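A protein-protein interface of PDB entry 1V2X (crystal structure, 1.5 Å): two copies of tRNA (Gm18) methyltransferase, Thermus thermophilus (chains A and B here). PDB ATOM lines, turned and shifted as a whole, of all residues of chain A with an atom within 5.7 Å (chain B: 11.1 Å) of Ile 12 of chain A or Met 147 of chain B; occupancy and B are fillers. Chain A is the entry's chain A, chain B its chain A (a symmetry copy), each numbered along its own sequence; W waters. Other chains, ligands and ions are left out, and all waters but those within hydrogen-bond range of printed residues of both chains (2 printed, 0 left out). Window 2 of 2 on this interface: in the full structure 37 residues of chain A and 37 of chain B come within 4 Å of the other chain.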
ATOM      1  N   ALA A   7      -0.708  19.518 -14.587  1.00  0.00           N
ATOM      2  CA  ALA A   7       0.204  18.399 -14.409  1.00  0.00           C
ATOM      3  C   ALA A   7       1.599  18.619 -14.979  1.00  0.00           C
ATOM      4  O   ALA A   7       2.507  19.056 -14.274  1.00  0.00           O
ATOM      5  CB  ALA A   7      -0.409  17.134 -15.004  1.00  0.00           C
ATOM      6  N   ARG A   8       1.757  18.295 -16.257  1.00  0.00           N
ATOM      7  CA  ARG A   8       3.027  18.424 -16.942  1.00  0.00           C
ATOM      8  C   ARG A   8       3.691  19.752 -16.601  1.00  0.00           C
ATOM      9  O   ARG A   8       4.802  19.785 -16.078  1.00  0.00           O
ATOM     10  CB  ARG A   8       2.805  18.319 -18.451  1.00  0.00           C
ATOM     11  CG  ARG A   8       4.072  18.072 -19.238  1.00  0.00           C
ATOM     12  CD  ARG A   8       3.865  18.299 -20.732  1.00  0.00           C
ATOM     13  NE  ARG A   8       5.139  18.273 -21.453  1.00  0.00           N
ATOM     14  CZ  ARG A   8       5.432  19.056 -22.490  1.00  0.00           C
ATOM     15  NH1 ARG A   8       4.539  19.933 -22.938  1.00  0.00           N
ATOM     16  NH2 ARG A   8       6.624  18.974 -23.071  1.00  0.00           N
ATOM     17  N   ARG A   9       2.984  20.840 -16.891  1.00  0.00           N
ATOM     18  CA  ARG A   9       3.463  22.191 -16.652  1.00  0.00           C
ATOM     19  C   ARG A   9       3.980  22.428 -15.227  1.00  0.00           C
ATOM     20  O   ARG A   9       5.112  22.869 -15.045  1.00  0.00           O
ATOM     21  CB  ARG A   9       2.343  23.186 -16.986  1.00  0.00           C
ATOM     22  CG  ARG A   9       2.677  24.648 -16.717  1.00  0.00           C
ATOM     23  CD  ARG A   9       4.110  24.938 -17.109  1.00  0.00           C
ATOM     24  NE  ARG A   9       4.539  26.277 -16.716  1.00  0.00           N
ATOM     25  CZ  ARG A   9       4.424  27.355 -17.486  1.00  0.00           C
ATOM     26  NH1 ARG A   9       3.889  27.262 -18.699  1.00  0.00           N
ATOM     27  NH2 ARG A   9       4.876  28.519 -17.048  1.00  0.00           N
ATOM     28  N   ARG A  10       3.151  22.126 -14.234  1.00  0.00           N
ATOM     29  CA  ARG A  10       3.486  22.313 -12.816  1.00  0.00           C
ATOM     30  C   ARG A  10       4.615  21.411 -12.309  1.00  0.00           C
ATOM     31  O   ARG A  10       5.505  21.889 -11.601  1.00  0.00           O
ATOM     32  CB  ARG A  10       2.216  22.123 -11.956  1.00  0.00           C
ATOM     33  CG  ARG A  10       2.354  21.285 -10.657  1.00  0.00           C
ATOM     34  CD  ARG A  10       0.940  20.880 -10.162  1.00  0.00           C
ATOM     35  NE  ARG A  10       0.880  20.003  -8.985  1.00  0.00           N
ATOM     36  CZ  ARG A  10      -0.163  19.212  -8.701  1.00  0.00           C
ATOM     37  NH1 ARG A  10      -1.218  19.184  -9.510  1.00  0.00           N
ATOM     38  NH2 ARG A  10      -0.171  18.460  -7.602  1.00  0.00           N
ATOM     39  N   ARG A  11       4.598  20.123 -12.651  1.00  0.00           N
ATOM     40  CA  ARG A  11       5.665  19.244 -12.178  1.00  0.00           C
ATOM     41  C   ARG A  11       7.024  19.603 -12.793  1.00  0.00           C
ATOM     42  O   ARG A  11       8.047  19.541 -12.121  1.00  0.00           O
ATOM     43  CB  ARG A  11       5.360  17.765 -12.469  1.00  0.00           C
ATOM     44  CG  ARG A  11       5.997  17.241 -13.740  1.00  0.00           C
ATOM     45  CD  ARG A  11       6.174  15.736 -13.706  1.00  0.00           C
ATOM     46  NE  ARG A  11       7.350  15.351 -12.936  1.00  0.00           N
ATOM     47  CZ  ARG A  11       7.771  14.098 -12.801  1.00  0.00           C
ATOM     48  NH1 ARG A  11       7.102  13.110 -13.384  1.00  0.00           N
ATOM     49  NH2 ARG A  11       8.869  13.833 -12.101  1.00  0.00           N
ATOM     50  N   ILE A  12       7.041  19.979 -14.068  1.00  0.00           N
ATOM     51  CA  ILE A  12       8.291  20.341 -14.717  1.00  0.00           C
ATOM     52  C   ILE A  12       8.921  21.602 -14.096  1.00  0.00           C
ATOM     53  O   ILE A  12      10.148  21.707 -13.949  1.00  0.00           O
ATOM     54  CB  ILE A  12       8.072  20.596 -16.233  1.00  0.00           C
ATOM     55  CG1 ILE A  12       7.858  19.273 -16.975  1.00  0.00           C
ATOM     56  CG2 ILE A  12       9.239  21.385 -16.787  1.00  0.00           C
ATOM     57  CD1 ILE A  12       7.417  19.435 -18.437  1.00  0.00           C
ATOM     58  N   GLU A  13       8.087  22.571 -13.747  1.00  0.00           N
ATOM     59  CA  GLU A  13       8.627  23.797 -13.190  1.00  0.00           C
ATOM     60  C   GLU A  13       9.090  23.488 -11.796  1.00  0.00           C
ATOM     61  O   GLU A  13      10.101  24.018 -11.355  1.00  0.00           O
ATOM     62  CB  GLU A  13       7.568  24.890 -13.119  1.00  0.00           C
ATOM     63  CG  GLU A  13       7.263  25.566 -14.401  1.00  0.00           C
ATOM     64  CD  GLU A  13       6.666  26.944 -14.159  1.00  0.00           C
ATOM     65  OE1 GLU A  13       7.400  27.854 -13.689  1.00  0.00           O
ATOM     66  OE2 GLU A  13       5.468  27.096 -14.428  1.00  0.00           O
ATOM     67  N   GLU A  14       8.346  22.646 -11.098  1.00  0.00           N
ATOM     68  CA  GLU A  14       8.731  22.289  -9.736  1.00  0.00           C
ATOM     69  C   GLU A  14      10.161  21.771  -9.732  1.00  0.00           C
ATOM     70  O   GLU A  14      10.970  22.149  -8.885  1.00  0.00           O
ATOM     71  CB  GLU A  14       7.798  21.240  -9.138  1.00  0.00           C
ATOM     72  CG  GLU A  14       7.481  21.531  -7.682  1.00  0.00           C
ATOM     73  CD  GLU A  14       7.507  20.300  -6.797  1.00  0.00           C
ATOM     74  OE1 GLU A  14       6.913  20.345  -5.694  1.00  0.00           O
ATOM     75  OE2 GLU A  14       8.126  19.291  -7.196  1.00  0.00           O
ATOM     76  N   VAL A  15      10.469  20.903 -10.683  1.00  0.00           N
ATOM     77  CA  VAL A  15      11.800  20.349 -10.810  1.00  0.00           C
ATOM     78  C   VAL A  15      12.826  21.369 -11.308  1.00  0.00           C
ATOM     79  O   VAL A  15      13.981  21.391 -10.858  1.00  0.00           O
ATOM     80  CB  VAL A  15      11.766  19.152 -11.776  1.00  0.00           C
ATOM     81  CG1 VAL A  15      13.164  18.655 -12.065  1.00  0.00           C
ATOM     82  CG2 VAL A  15      10.901  18.081 -11.189  1.00  0.00           C
ATOM     83  N   LEU A  16      12.405  22.242 -12.229  1.00  0.00           N
ATOM     84  CA  LEU A  16      13.305  23.244 -12.753  1.00  0.00           C
ATOM     85  C   LEU A  16      13.739  24.169 -11.619  1.00  0.00           C
ATOM     86  O   LEU A  16      14.851  24.708 -11.618  1.00  0.00           O
ATOM     87  CB  LEU A  16      12.582  24.077 -13.806  1.00  0.00           C
ATOM     88  CG  LEU A  16      13.306  24.447 -15.078  1.00  0.00           C
ATOM     89  CD1 LEU A  16      12.579  25.624 -15.748  1.00  0.00           C
ATOM     90  CD2 LEU A  16      14.734  24.763 -14.778  1.00  0.00           C
ATOM     91  N   ARG A  17      12.844  24.338 -10.659  1.00  0.00           N
ATOM     92  CA  ARG A  17      13.104  25.212  -9.510  1.00  0.00           C
ATOM     93  C   ARG A  17      14.139  24.655  -8.542  1.00  0.00           C
ATOM     94  O   ARG A  17      14.625  25.369  -7.659  1.00  0.00           O
ATOM     95  CB  ARG A  17      11.786  25.523  -8.781  1.00  0.00           C
ATOM     96  CG  ARG A  17      10.869  26.506  -9.516  1.00  0.00           C
ATOM     97  CD  ARG A  17       9.543  26.600  -8.804  1.00  0.00           C
ATOM     98  NE  ARG A  17       9.608  27.493  -7.639  1.00  0.00           N
ATOM     99  CZ  ARG A  17       9.586  28.826  -7.720  1.00  0.00           C
ATOM    100  NH1 ARG A  17       9.498  29.425  -8.898  1.00  0.00           N
ATOM    101  NH2 ARG A  17       9.677  29.564  -6.619  1.00  0.00           N
ATOM    102  N   ARG A  19      16.877  23.040  -9.890  1.00  0.00           N
ATOM    103  CA  ARG A  19      18.117  22.881 -10.648  1.00  0.00           C
ATOM    104  C   ARG A  19      19.247  23.755 -10.112  1.00  0.00           C
ATOM    105  O   ARG A  19      19.021  24.924  -9.797  1.00  0.00           O
ATOM    106  CB  ARG A  19      17.887  23.173 -12.125  1.00  0.00           C
ATOM    107  CG  ARG A  19      17.198  22.005 -12.864  1.00  0.00           C
ATOM    108  CD  ARG A  19      18.084  20.790 -12.795  1.00  0.00           C
ATOM    109  NE  ARG A  19      17.932  19.784 -13.877  1.00  0.00           N
ATOM    110  CZ  ARG A  19      17.508  18.537 -13.659  1.00  0.00           C
ATOM    111  NH1 ARG A  19      17.127  18.131 -12.450  1.00  0.00           N
ATOM    112  NH2 ARG A  19      17.621  17.619 -14.604  1.00  0.00           N
ATOM    113  N   ASP A  44      20.646  14.173 -12.775  1.00  0.00           N
ATOM    114  CA  ASP A  44      19.249  14.637 -12.713  1.00  0.00           C
ATOM    115  C   ASP A  44      18.682  14.557 -11.277  1.00  0.00           C
ATOM    116  O   ASP A  44      18.046  15.497 -10.767  1.00  0.00           O
ATOM    117  CB  ASP A  44      18.346  13.779 -13.584  1.00  0.00           C
ATOM    118  CG  ASP A  44      16.872  14.146 -13.415  1.00  0.00           C
ATOM    119  OD1 ASP A  44      16.449  15.225 -13.911  1.00  0.00           O
ATOM    120  OD2 ASP A  44      16.133  13.362 -12.778  1.00  0.00           O
ATOM    121  N   TRP A  73      16.814  15.270 -20.043  1.00  0.00           N
ATOM    122  CA  TRP A  73      16.744  16.380 -19.077  1.00  0.00           C
ATOM    123  C   TRP A  73      18.016  17.055 -18.600  1.00  0.00           C
ATOM    124  O   TRP A  73      17.984  18.220 -18.122  1.00  0.00           O
ATOM    125  CB  TRP A  73      15.993  15.923 -17.829  1.00  0.00           C
ATOM    126  CG  TRP A  73      14.834  15.069 -18.119  1.00  0.00           C
ATOM    127  CD1 TRP A  73      14.779  13.707 -18.045  1.00  0.00           C
ATOM    128  CD2 TRP A  73      13.566  15.503 -18.586  1.00  0.00           C
ATOM    129  NE1 TRP A  73      13.545  13.264 -18.447  1.00  0.00           N
ATOM    130  CE2 TRP A  73      12.778  14.349 -18.786  1.00  0.00           C
ATOM    131  CE3 TRP A  73      13.009  16.762 -18.857  1.00  0.00           C
ATOM    132  CZ2 TRP A  73      11.453  14.413 -19.250  1.00  0.00           C
ATOM    133  CZ3 TRP A  73      11.684  16.827 -19.320  1.00  0.00           C
ATOM    134  CH2 TRP A  73      10.928  15.656 -19.510  1.00  0.00           C
ATOM    135  N   LEU A 188      12.849  25.970 -19.168  1.00  0.00           N
ATOM    136  CA  LEU A 188      11.439  25.658 -19.003  1.00  0.00           C
ATOM    137  C   LEU A 188      10.889  25.387 -20.401  1.00  0.00           C
ATOM    138  O   LEU A 188      10.122  24.455 -20.612  1.00  0.00           O
ATOM    139  CB  LEU A 188      10.703  26.836 -18.343  1.00  0.00           C
ATOM    140  CG  LEU A 188       9.189  26.640 -18.148  1.00  0.00           C
ATOM    141  CD1 LEU A 188       8.946  25.298 -17.494  1.00  0.00           C
ATOM    142  CD2 LEU A 188       8.597  27.766 -17.283  1.00  0.00           C
ATOM    143  N   TRP A 191      12.104  21.640 -21.804  1.00  0.00           N
ATOM    144  CA  TRP A 191      11.409  20.563 -21.122  1.00  0.00           C
ATOM    145  C   TRP A 191       9.930  20.562 -21.523  1.00  0.00           C
ATOM    146  O   TRP A 191       9.460  21.600 -22.038  1.00  0.00           O
ATOM    147  CB  TRP A 191      11.552  20.737 -19.620  1.00  0.00           C
ATOM    148  CG  TRP A 191      12.958  20.539 -19.123  1.00  0.00           C
ATOM    149  CD1 TRP A 191      14.101  20.416 -19.871  1.00  0.00           C
ATOM    150  CD2 TRP A 191      13.355  20.430 -17.759  1.00  0.00           C
ATOM    151  NE1 TRP A 191      15.191  20.232 -19.042  1.00  0.00           N
ATOM    152  CE2 TRP A 191      14.752  20.241 -17.740  1.00  0.00           C
ATOM    153  CE3 TRP A 191      12.656  20.477 -16.540  1.00  0.00           C
ATOM    154  CZ2 TRP A 191      15.476  20.098 -16.541  1.00  0.00           C
ATOM    155  CZ3 TRP A 191      13.364  20.336 -15.360  1.00  0.00           C
ATOM    156  CH2 TRP A 191      14.765  20.148 -15.370  1.00  0.00           C
ATOM    157  N   LEU B 101      10.299   3.167  -4.505  1.00  0.00           N
ATOM    158  CA  LEU B 101      10.173   4.463  -5.143  1.00  0.00           C
ATOM    159  C   LEU B 101       8.883   5.167  -4.718  1.00  0.00           C
ATOM    160  O   LEU B 101       8.596   6.263  -5.179  1.00  0.00           O
ATOM    161  CB  LEU B 101      10.260   4.292  -6.669  1.00  0.00           C
ATOM    162  CG  LEU B 101      11.673   4.107  -7.271  1.00  0.00           C
ATOM    163  CD1 LEU B 101      12.444   5.402  -7.110  1.00  0.00           C
ATOM    164  CD2 LEU B 101      12.447   2.998  -6.611  1.00  0.00           C
ATOM    165  N   GLU B 103       6.169   7.232  -2.490  1.00  0.00           N
ATOM    166  CA  GLU B 103       6.392   8.471  -1.767  1.00  0.00           C
ATOM    167  C   GLU B 103       6.143   8.303  -0.264  1.00  0.00           C
ATOM    168  O   GLU B 103       6.373   9.221   0.512  1.00  0.00           O
ATOM    169  CB  GLU B 103       5.556   9.593  -2.378  1.00  0.00           C
ATOM    170  CG  GLU B 103       5.977   9.868  -3.817  1.00  0.00           C
ATOM    171  CD  GLU B 103       6.398  11.315  -4.075  1.00  0.00           C
ATOM    172  OE1 GLU B 103       7.039  11.570  -5.124  1.00  0.00           O
ATOM    173  OE2 GLU B 103       6.082  12.196  -3.243  1.00  0.00           O
ATOM    174  N   LYS B 141      13.719   5.176   0.889  1.00  0.00           N
ATOM    175  CA  LYS B 141      13.909   5.786  -0.428  1.00  0.00           C
ATOM    176  C   LYS B 141      14.997   6.850  -0.452  1.00  0.00           C
ATOM    177  O   LYS B 141      15.294   7.498   0.554  1.00  0.00           O
ATOM    178  CB  LYS B 141      12.586   6.389  -0.926  1.00  0.00           C
ATOM    179  CG  LYS B 141      12.715   7.082  -2.285  1.00  0.00           C
ATOM    180  CD  LYS B 141      11.407   7.720  -2.760  1.00  0.00           C
ATOM    181  CE  LYS B 141      11.640   8.332  -4.139  1.00  0.00           C
ATOM    182  NZ  LYS B 141      10.371   8.711  -4.785  1.00  0.00           N
ATOM    183  N   PRO B 143      16.028  10.432  -1.906  1.00  0.00           N
ATOM    184  CA  PRO B 143      15.374  11.606  -2.534  1.00  0.00           C
ATOM    185  C   PRO B 143      15.770  11.820  -3.995  1.00  0.00           C
ATOM    186  O   PRO B 143      16.965  11.817  -4.341  1.00  0.00           O
ATOM    187  CB  PRO B 143      15.847  12.774  -1.676  1.00  0.00           C
ATOM    188  CG  PRO B 143      16.187  12.161  -0.357  1.00  0.00           C
ATOM    189  CD  PRO B 143      16.805  10.827  -0.716  1.00  0.00           C
ATOM    190  N   MET B 144      14.772  12.034  -4.844  1.00  0.00           N
ATOM    191  CA  MET B 144      15.018  12.265  -6.267  1.00  0.00           C
ATOM    192  C   MET B 144      14.501  13.677  -6.510  1.00  0.00           C
ATOM    193  O   MET B 144      13.296  13.909  -6.433  1.00  0.00           O
ATOM    194  CB  MET B 144      14.224  11.268  -7.103  1.00  0.00           C
ATOM    195  CG  MET B 144      14.553   9.777  -6.830  1.00  0.00           C
ATOM    196  SD  MET B 144      16.172   9.339  -7.405  1.00  0.00           S
ATOM    197  CE  MET B 144      17.046   9.442  -5.916  1.00  0.00           C
ATOM    198  N   LEU B 145      15.407  14.607  -6.820  1.00  0.00           N
ATOM    199  CA  LEU B 145      15.032  15.996  -6.996  1.00  0.00           C
ATOM    200  C   LEU B 145      14.912  16.454  -8.431  1.00  0.00           C
ATOM    201  O   LEU B 145      14.786  17.648  -8.673  1.00  0.00           O
ATOM    202  CB  LEU B 145      16.039  16.887  -6.244  1.00  0.00           C
ATOM    203  CG  LEU B 145      16.272  16.439  -4.792  1.00  0.00           C
ATOM    204  CD1 LEU B 145      17.351  17.307  -4.183  1.00  0.00           C
ATOM    205  CD2 LEU B 145      14.973  16.549  -3.982  1.00  0.00           C
ATOM    206  N   GLY B 146      14.935  15.508  -9.377  1.00  0.00           N
ATOM    207  CA  GLY B 146      14.839  15.875 -10.777  1.00  0.00           C
ATOM    208  C   GLY B 146      13.621  15.288 -11.476  1.00  0.00           C
ATOM    209  O   GLY B 146      12.580  15.016 -10.860  1.00  0.00           O
ATOM    210  N   MET B 147      13.749  15.135 -12.792  1.00  0.00           N
ATOM    211  CA  MET B 147      12.665  14.601 -13.583  1.00  0.00           C
ATOM    212  C   MET B 147      12.564  13.069 -13.584  1.00  0.00           C
ATOM    213  O   MET B 147      11.474  12.551 -13.743  1.00  0.00           O
ATOM    214  CB  MET B 147      12.767  15.087 -15.034  1.00  0.00           C
ATOM    215  CG  MET B 147      12.389  16.549 -15.244  1.00  0.00           C
ATOM    216  SD  MET B 147      10.662  16.868 -14.844  1.00  0.00           S
ATOM    217  CE  MET B 147       9.923  16.022 -16.190  1.00  0.00           C
ATOM    218  N   VAL B 148      13.675  12.351 -13.415  1.00  0.00           N
ATOM    219  CA  VAL B 148      13.573  10.897 -13.453  1.00  0.00           C
ATOM    220  C   VAL B 148      13.074  10.357 -12.134  1.00  0.00           C
ATOM    221  O   VAL B 148      13.241  10.974 -11.068  1.00  0.00           O
ATOM    222  CB  VAL B 148      14.878  10.182 -13.864  1.00  0.00           C
ATOM    223  CG1 VAL B 148      15.357  10.719 -15.231  1.00  0.00           C
ATOM    224  CG2 VAL B 148      15.919  10.309 -12.774  1.00  0.00           C
ATOM    225  N   GLN B 149      12.402   9.214 -12.247  1.00  0.00           N
ATOM    226  CA  GLN B 149      11.751   8.523 -11.146  1.00  0.00           C
ATOM    227  C   GLN B 149      12.651   7.632 -10.313  1.00  0.00           C
ATOM    228  O   GLN B 149      12.416   7.437  -9.120  1.00  0.00           O
ATOM    229  CB  GLN B 149      10.594   7.691 -11.727  1.00  0.00           C
ATOM    230  CG  GLN B 149      10.564   7.657 -13.293  1.00  0.00           C
ATOM    231  CD  GLN B 149      11.763   6.941 -13.961  1.00  0.00           C
ATOM    232  OE1 GLN B 149      12.367   7.463 -14.910  1.00  0.00           O
ATOM    233  NE2 GLN B 149      12.089   5.737 -13.480  1.00  0.00           N
ATOM    234  N   SER B 150      13.696   7.100 -10.924  1.00  0.00           N
ATOM    235  CA  SER B 150      14.596   6.219 -10.175  1.00  0.00           C
ATOM    236  C   SER B 150      16.042   6.305 -10.597  1.00  0.00           C
ATOM    237  O   SER B 150      16.376   6.806 -11.700  1.00  0.00           O
ATOM    238  CB  SER B 150      14.145   4.777 -10.358  1.00  0.00           C
ATOM    239  OG  SER B 150      14.236   4.497 -11.734  1.00  0.00           O
ATOM    240  N   LEU B 151      16.906   5.754  -9.749  1.00  0.00           N
ATOM    241  CA  LEU B 151      18.339   5.702 -10.018  1.00  0.00           C
ATOM    242  C   LEU B 151      18.691   4.300 -10.540  1.00  0.00           C
ATOM    243  O   LEU B 151      17.895   3.349 -10.427  1.00  0.00           O
ATOM    244  CB  LEU B 151      19.140   5.887  -8.727  1.00  0.00           C
ATOM    245  CG  LEU B 151      19.040   7.226  -8.011  1.00  0.00           C
ATOM    246  CD1 LEU B 151      19.540   7.036  -6.582  1.00  0.00           C
ATOM    247  CD2 LEU B 151      19.879   8.297  -8.797  1.00  0.00           C
HETATM  248  O   HOH W   1      15.174  12.859 -10.130  1.00  0.00           O
HETATM  249  O   HOH W   2      16.000  19.554 -10.337  1.00  0.00           O
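Among the printed residues, pairs that only touch across the chains: Ile 12 of chain A with Met 147 of chain B (3.9 Å), Val 15 of chain A with Leu 145 of chain B (3.9 Å), Val 15 of chain A with Gly 146 of chain B (3.4 Å), Val 15 of chain A with Met 147 of chain B (3.6 Å), Arg 19 of chain A with Gly 146 of chain B (3.6 Å), Trp 73 of chain A with Met 147 of chain B (3.5 Å) and Trp 191 of chain A with Met 147 of chain B (3.9 Å).
O of Met 147 of chain B sits at hydrogen-bond distance from NH2 of Arg 11 of chain A, at 3.3 Å.
OD2 of Asp 44 of chain A sits at hydrogen-bond distance from N of Val 148 of chain B.
The backbone NH (N) of Gly 146 of chain B lies close to the backbone carbonyl oxygen (O) of Asp 44 of chain A (3.4 Å).
The side-chain carboxylate (OD1) of Asp 44 of chain A sits at hydrogen-bond distance from the backbone NH (N) of Met 147 of chain B (2.9 Å).
The guanidinium group of Arg 19 of chain A is in salt-bridge range of the side-chain carboxylate of Asp 44 of chain A (2.8 Å).
No position is printed for both chains.
Of the 16 printed residues of chain A, 7 touch a printed residue of chain B.
Hydrophobic or aromatic side chains of chain A within 4 Å of the printed part of chain B: Ile 12, Val 15, Trp 73 and Trp 191.
Hydrophobic or aromatic side chains of chain B that line the printed part of chain A: Met 147 and Val 148.
Along chain B the printed residues that touch a printed residue of chain A span positions 145 to 148.
No residue of chain B comes within 4 Å of Arg 8 of chain A.
Arg 10 of chain A touches none of the printed residues of chain B.
Of the printed residues of chain B, Arg 11 of chain A touches Met 147.
Ile 12 of chain A touches just one residue of chain B: Met 147.
Val 15 of chain A touches just these residues of chain B: Leu 145, Gly 146 and Met 147.
No residue of chain B comes within 4 Å of Leu 16 of chain A.
Printed residues of chain B within 4 Å of Arg 19 of chain A: Gly 146 (3.6 Å).
Asp 44 of chain A touches just these residues of chain B: Gly 146, Met 147 and Val 148.
Trp 73 of chain A touches one residue of chain B.
No residue of chain B comes within 4 Å of Leu 188 of chain A.
Lys 141 of chain B touches none of the printed residues of chain A.
Of the printed residues of chain A, Leu 145 of chain B touches Val 15.
Of the printed residues of chain A, Gly 146 of chain B touches Val 15, Arg 19 and Asp 44.
Of chain A, only Arg 11, Ile 12, Val 15, Asp 44, Trp 73 and Trp 191 come within 4 Å of Met 147 of chain B.
Of the printed residues of chain A, Val 148 of chain B touches Asp 44.
The nearest residue of chain B that does not touch Ile 12 of chain A is Gly 146 of chain B (7.7 Å).
Water W1 lies within hydrogen-bond range of the backbone NH (N) of Gly 146 of chain B (2.8 Å), the backbone carbonyl oxygen (O) of Val 148 of chain B (2.9 Å) and the side-chain carboxylate (OD2) of Asp 44 of chain A (2.9 Å).
Water W2 lies within hydrogen-bond range of O of Val 15 of chain A (2.8 Å), NH1 of Arg 19 of chain A (2.8 Å) and O of Leu 145 of chain B (2.8 Å).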
